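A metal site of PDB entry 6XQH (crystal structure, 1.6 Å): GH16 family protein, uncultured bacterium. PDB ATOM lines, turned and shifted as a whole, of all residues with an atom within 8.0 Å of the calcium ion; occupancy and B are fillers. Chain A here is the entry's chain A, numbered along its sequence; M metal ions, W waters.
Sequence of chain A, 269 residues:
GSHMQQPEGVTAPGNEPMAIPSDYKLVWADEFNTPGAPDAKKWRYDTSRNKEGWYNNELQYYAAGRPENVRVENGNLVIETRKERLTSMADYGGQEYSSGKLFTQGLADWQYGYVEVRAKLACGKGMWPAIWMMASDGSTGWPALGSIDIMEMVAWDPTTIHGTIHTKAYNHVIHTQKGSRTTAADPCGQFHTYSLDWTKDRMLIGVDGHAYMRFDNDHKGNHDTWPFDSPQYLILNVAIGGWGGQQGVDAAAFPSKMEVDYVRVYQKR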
ATOM      1  N   ASP A  30      28.050 -28.316 -22.187  1.00  0.00           N
ATOM      2  CA  ASP A  30      26.940 -27.385 -22.116  1.00  0.00           C
ATOM      3  C   ASP A  30      25.953 -28.025 -21.152  1.00  0.00           C
ATOM      4  O   ASP A  30      25.393 -29.052 -21.479  1.00  0.00           O
ATOM      5  CB  ASP A  30      26.358 -27.026 -23.470  1.00  0.00           C
ATOM      6  CG  ASP A  30      25.569 -25.748 -23.347  1.00  0.00           C
ATOM      7  OD1 ASP A  30      25.189 -25.392 -22.240  1.00  0.00           O
ATOM      8  OD2 ASP A  30      25.338 -25.097 -24.392  1.00  0.00           O
ATOM      9  N   GLU A  31      25.826 -27.408 -20.025  1.00  0.00           N
ATOM     10  CA  GLU A  31      24.851 -27.860 -19.021  1.00  0.00           C
ATOM     11  C   GLU A  31      23.505 -27.192 -19.299  1.00  0.00           C
ATOM     12  O   GLU A  31      22.561 -27.539 -18.569  1.00  0.00           O
ATOM     13  CB  GLU A  31      25.370 -27.497 -17.637  1.00  0.00           C
ATOM     14  CG  GLU A  31      26.773 -28.038 -17.341  1.00  0.00           C
ATOM     15  CD  GLU A  31      26.772 -29.505 -16.947  1.00  0.00           C
ATOM     16  OE1 GLU A  31      25.647 -30.071 -16.809  1.00  0.00           O
ATOM     17  OE2 GLU A  31      27.838 -30.086 -16.803  1.00  0.00           O
ATOM     18  N   PHE A  32      23.428 -26.223 -20.211  1.00  0.00           N
ATOM     19  CA  PHE A  32      22.164 -25.507 -20.492  1.00  0.00           C
ATOM     20  C   PHE A  32      21.660 -24.838 -19.208  1.00  0.00           C
ATOM     21  O   PHE A  32      20.471 -24.789 -18.935  1.00  0.00           O
ATOM     22  CB  PHE A  32      21.164 -26.450 -21.147  1.00  0.00           C
ATOM     23  CG  PHE A  32      21.699 -26.990 -22.439  1.00  0.00           C
ATOM     24  CD1 PHE A  32      21.958 -26.170 -23.547  1.00  0.00           C
ATOM     25  CD2 PHE A  32      22.033 -28.317 -22.539  1.00  0.00           C
ATOM     26  CE1 PHE A  32      22.532 -26.679 -24.691  1.00  0.00           C
ATOM     27  CE2 PHE A  32      22.563 -28.835 -23.696  1.00  0.00           C
ATOM     28  CZ  PHE A  32      22.774 -28.054 -24.787  1.00  0.00           C
ATOM     29  N   ASN A  33      22.590 -24.205 -18.519  1.00  0.00           N
ATOM     30  CA  ASN A  33      22.340 -23.513 -17.241  1.00  0.00           C
ATOM     31  C   ASN A  33      21.652 -22.167 -17.449  1.00  0.00           C
ATOM     32  O   ASN A  33      21.173 -21.598 -16.503  1.00  0.00           O
ATOM     33  CB  ASN A  33      23.663 -23.233 -16.539  1.00  0.00           C
ATOM     34  CG  ASN A  33      24.296 -24.426 -15.841  1.00  0.00           C
ATOM     35  OD1 ASN A  33      23.654 -25.451 -15.642  1.00  0.00           O
ATOM     36  ND2 ASN A  33      25.525 -24.201 -15.358  1.00  0.00           N
ATOM     37  N   THR A  34      21.766 -21.587 -18.647  1.00  0.00           N
ATOM     38  CA  THR A  34      21.394 -20.163 -18.809  1.00  0.00           C
ATOM     39  C   THR A  34      20.166 -20.074 -19.689  1.00  0.00           C
ATOM     40  O   THR A  34      20.228 -20.316 -20.870  1.00  0.00           O
ATOM     41  CB  THR A  34      22.555 -19.380 -19.409  1.00  0.00           C
ATOM     42  OG1 THR A  34      23.695 -19.555 -18.558  1.00  0.00           O
ATOM     43  CG2 THR A  34      22.185 -17.944 -19.611  1.00  0.00           C
ATOM     44  N   VAL A  72      16.525 -22.447 -24.277  1.00  0.00           N
ATOM     45  CA  VAL A  72      17.060 -23.069 -23.033  1.00  0.00           C
ATOM     46  C   VAL A  72      16.085 -22.714 -21.944  1.00  0.00           C
ATOM     47  O   VAL A  72      15.785 -21.513 -21.767  1.00  0.00           O
ATOM     48  CB  VAL A  72      18.508 -22.671 -22.694  1.00  0.00           C
ATOM     49  CG1 VAL A  72      18.941 -23.235 -21.355  1.00  0.00           C
ATOM     50  CG2 VAL A  72      19.489 -23.085 -23.798  1.00  0.00           C
ATOM     51  N   GLU A  73      15.513 -23.746 -21.331  1.00  0.00           N
ATOM     52  CA  GLU A  73      14.486 -23.578 -20.285  1.00  0.00           C
ATOM     53  C   GLU A  73      14.769 -24.594 -19.202  1.00  0.00           C
ATOM     54  O   GLU A  73      14.901 -25.778 -19.571  1.00  0.00           O
ATOM     55  CB  GLU A  73      13.056 -23.922 -20.696  1.00  0.00           C
ATOM     56  CG  GLU A  73      12.412 -22.927 -21.588  1.00  0.00           C
ATOM     57  CD  GLU A  73      11.024 -23.358 -22.084  1.00  0.00           C
ATOM     58  OE1 GLU A  73      10.683 -24.535 -21.841  1.00  0.00           O
ATOM     59  OE2 GLU A  73      10.386 -22.579 -22.716  1.00  0.00           O
ATOM     60  N   ASN A  74      14.795 -24.158 -17.954  1.00  0.00           N
ATOM     61  CA  ASN A  74      14.819 -25.013 -16.749  1.00  0.00           C
ATOM     62  C   ASN A  74      15.943 -26.032 -16.849  1.00  0.00           C
ATOM     63  O   ASN A  74      15.694 -27.222 -16.604  1.00  0.00           O
ATOM     64  CB  ASN A  74      13.441 -25.663 -16.598  1.00  0.00           C
ATOM     65  CG  ASN A  74      12.350 -24.634 -16.331  1.00  0.00           C
ATOM     66  OD1 ASN A  74      11.381 -24.557 -17.129  1.00  0.00           O
ATOM     67  ND2 ASN A  74      12.474 -23.818 -15.291  1.00  0.00           N
ATOM     68  N   GLY A  75      17.094 -25.598 -17.307  1.00  0.00           N
ATOM     69  CA  GLY A  75      18.267 -26.464 -17.325  1.00  0.00           C
ATOM     70  C   GLY A  75      18.339 -27.377 -18.501  1.00  0.00           C
ATOM     71  O   GLY A  75      19.321 -28.124 -18.565  1.00  0.00           O
ATOM     72  N   ASN A  76      17.458 -27.242 -19.486  1.00  0.00           N
ATOM     73  CA  ASN A  76      17.477 -28.083 -20.677  1.00  0.00           C
ATOM     74  C   ASN A  76      17.514 -27.227 -21.934  1.00  0.00           C
ATOM     75  O   ASN A  76      16.862 -26.183 -21.975  1.00  0.00           O
ATOM     76  CB  ASN A  76      16.236 -28.982 -20.793  1.00  0.00           C
ATOM     77  CG  ASN A  76      16.075 -29.880 -19.597  1.00  0.00           C
ATOM     78  OD1 ASN A  76      17.033 -30.452 -19.064  1.00  0.00           O
ATOM     79  ND2 ASN A  76      14.880 -29.889 -19.031  1.00  0.00           N
ATOM     80  N   LEU A  77      18.266 -27.703 -22.896  1.00  0.00           N
ATOM     81  CA  LEU A  77      17.999 -27.272 -24.265  1.00  0.00           C
ATOM     82  C   LEU A  77      16.659 -27.850 -24.658  1.00  0.00           C
ATOM     83  O   LEU A  77      16.506 -29.078 -24.495  1.00  0.00           O
ATOM     84  CB  LEU A  77      19.110 -27.752 -25.164  1.00  0.00           C
ATOM     85  CG  LEU A  77      18.966 -27.349 -26.630  1.00  0.00           C
ATOM     86  CD1 LEU A  77      19.194 -25.845 -26.749  1.00  0.00           C
ATOM     87  CD2 LEU A  77      19.954 -28.108 -27.503  1.00  0.00           C
ATOM     88  N   ARG A 118      22.515 -36.262 -21.990  1.00  0.00           N
ATOM     89  CA  ARG A 118      21.354 -36.695 -21.214  1.00  0.00           C
ATOM     90  C   ARG A 118      20.146 -36.001 -21.834  1.00  0.00           C
ATOM     91  O   ARG A 118      20.118 -34.784 -21.881  1.00  0.00           O
ATOM     92  CB  ARG A 118      21.501 -36.336 -19.749  1.00  0.00           C
ATOM     93  CG  ARG A 118      20.313 -36.813 -18.898  1.00  0.00           C
ATOM     94  CD  ARG A 118      20.620 -36.740 -17.422  1.00  0.00           C
ATOM     95  NE  ARG A 118      19.562 -37.338 -16.625  1.00  0.00           N
ATOM     96  CZ  ARG A 118      18.564 -36.661 -16.052  1.00  0.00           C
ATOM     97  NH1 ARG A 118      18.438 -35.346 -16.196  1.00  0.00           N
ATOM     98  NH2 ARG A 118      17.680 -37.342 -15.294  1.00  0.00           N
ATOM     99  N   PHE A 191      14.378 -38.988 -19.144  1.00  0.00           N
ATOM    100  CA  PHE A 191      15.757 -38.830 -19.614  1.00  0.00           C
ATOM    101  C   PHE A 191      16.478 -40.165 -19.605  1.00  0.00           C
ATOM    102  O   PHE A 191      16.322 -41.016 -18.703  1.00  0.00           O
ATOM    103  CB  PHE A 191      16.517 -37.843 -18.726  1.00  0.00           C
ATOM    104  CG  PHE A 191      16.078 -36.436 -18.916  1.00  0.00           C
ATOM    105  CD1 PHE A 191      16.646 -35.679 -19.945  1.00  0.00           C
ATOM    106  CD2 PHE A 191      15.134 -35.888 -18.055  1.00  0.00           C
ATOM    107  CE1 PHE A 191      16.227 -34.380 -20.177  1.00  0.00           C
ATOM    108  CE2 PHE A 191      14.703 -34.588 -18.295  1.00  0.00           C
ATOM    109  CZ  PHE A 191      15.279 -33.851 -19.337  1.00  0.00           C
ATOM    110  N   VAL A 260      17.384 -31.573 -23.777  1.00  0.00           N
ATOM    111  CA  VAL A 260      18.740 -32.029 -23.517  1.00  0.00           C
ATOM    112  C   VAL A 260      19.216 -31.369 -22.228  1.00  0.00           C
ATOM    113  O   VAL A 260      19.366 -30.136 -22.145  1.00  0.00           O
ATOM    114  CB  VAL A 260      19.683 -31.707 -24.677  1.00  0.00           C
ATOM    115  CG1 VAL A 260      21.034 -32.320 -24.324  1.00  0.00           C
ATOM    116  CG2 VAL A 260      19.149 -32.222 -26.016  1.00  0.00           C
ATOM    117  N   ASP A 261      19.456 -32.198 -21.226  1.00  0.00           N
ATOM    118  CA  ASP A 261      19.844 -31.698 -19.901  1.00  0.00           C
ATOM    119  C   ASP A 261      21.298 -31.236 -19.957  1.00  0.00           C
ATOM    120  O   ASP A 261      21.633 -30.185 -19.431  1.00  0.00           O
ATOM    121  CB  ASP A 261      19.712 -32.826 -18.899  1.00  0.00           C
ATOM    122  CG  ASP A 261      20.064 -32.400 -17.489  1.00  0.00           C
ATOM    123  OD1 ASP A 261      20.248 -31.181 -17.179  1.00  0.00           O
ATOM    124  OD2 ASP A 261      20.122 -33.255 -16.638  1.00  0.00           O
ATOM    125  N   TYR A 262      22.127 -32.001 -20.656  1.00  0.00           N
ATOM    126  CA  TYR A 262      23.533 -31.593 -20.798  1.00  0.00           C
ATOM    127  C   TYR A 262      24.197 -32.367 -21.926  1.00  0.00           C
ATOM    128  O   TYR A 262      23.780 -33.455 -22.294  1.00  0.00           O
ATOM    129  CB  TYR A 262      24.284 -31.815 -19.477  1.00  0.00           C
ATOM    130  CG  TYR A 262      24.366 -33.230 -18.974  1.00  0.00           C
ATOM    131  CD1 TYR A 262      25.160 -34.167 -19.627  1.00  0.00           C
ATOM    132  CD2 TYR A 262      23.678 -33.638 -17.858  1.00  0.00           C
ATOM    133  CE1 TYR A 262      25.256 -35.460 -19.169  1.00  0.00           C
ATOM    134  CE2 TYR A 262      23.802 -34.934 -17.365  1.00  0.00           C
ATOM    135  CZ  TYR A 262      24.618 -35.831 -18.010  1.00  0.00           C
ATOM    136  OH  TYR A 262      24.761 -37.142 -17.623  1.00  0.00           O
ATOM    137  N   VAL A 263      25.273 -31.771 -22.369  1.00  0.00           N
ATOM    138  CA  VAL A 263      26.279 -32.421 -23.218  1.00  0.00           C
ATOM    139  C   VAL A 263      27.596 -32.334 -22.476  1.00  0.00           C
ATOM    140  O   VAL A 263      27.979 -31.254 -22.121  1.00  0.00           O
ATOM    141  CB  VAL A 263      26.353 -31.720 -24.584  1.00  0.00           C
ATOM    142  CG1 VAL A 263      27.547 -32.239 -25.368  1.00  0.00           C
ATOM    143  CG2 VAL A 263      25.050 -31.795 -25.359  1.00  0.00           C
ATOM    144  N   ARG A 264      28.266 -33.431 -22.228  1.00  0.00           N
ATOM    145  CA  ARG A 264      29.554 -33.402 -21.524  1.00  0.00           C
ATOM    146  C   ARG A 264      30.508 -34.191 -22.362  1.00  0.00           C
ATOM    147  O   ARG A 264      30.113 -35.287 -22.776  1.00  0.00           O
ATOM    148  CB  ARG A 264      29.388 -33.962 -20.121  1.00  0.00           C
ATOM    149  CG  ARG A 264      28.591 -33.061 -19.215  1.00  0.00           C
ATOM    150  CD  ARG A 264      28.395 -33.775 -17.897  1.00  0.00           C
ATOM    151  NE  ARG A 264      27.480 -32.996 -17.068  1.00  0.00           N
ATOM    152  CZ  ARG A 264      26.795 -33.449 -16.037  1.00  0.00           C
ATOM    153  NH1 ARG A 264      26.873 -34.715 -15.676  1.00  0.00           N
ATOM    154  NH2 ARG A 264      25.952 -32.659 -15.415  1.00  0.00           N
HETATM  155 CA    CA M   1      21.121 -28.989 -17.397  1.00  0.00          CA
HETATM  156  O   HOH W   1      22.949 -29.975 -16.232  1.00  0.00           O
HETATM  157  O   HOH W   2      21.367 -26.945 -16.004  1.00  0.00           O
HETATM  158  O   HOH W   3      19.588 -29.301 -15.449  1.00  0.00           O
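The guanidinium group (NE) of Arg 264 lies within salt-bridge range of the side-chain carboxylate (OE2) of Glu 31, at 2.9 Å.
NH1 of Arg 118 is in salt-bridge range of OD2 of Asp 261.
O of Gly 75 is bound to the calcium ion (2.3 Å).
O of Glu 31 binds the calcium ion (2.4 Å).
The side-chain carboxylate (OD1) of Asp 261 is bound to the calcium ion (2.4 Å).
The calcium ion is bound by water W1, at 2.4 Å.
The backbone carbonyl oxygen (O) of Asp 261 binds the calcium ion, 2.4 Å away.
The calcium ion is bound by water W2 (2.5 Å).
Water W3 is bound to the calcium ion, at 2.5 Å.
The calcium ion has seven donor atoms within binding distance.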
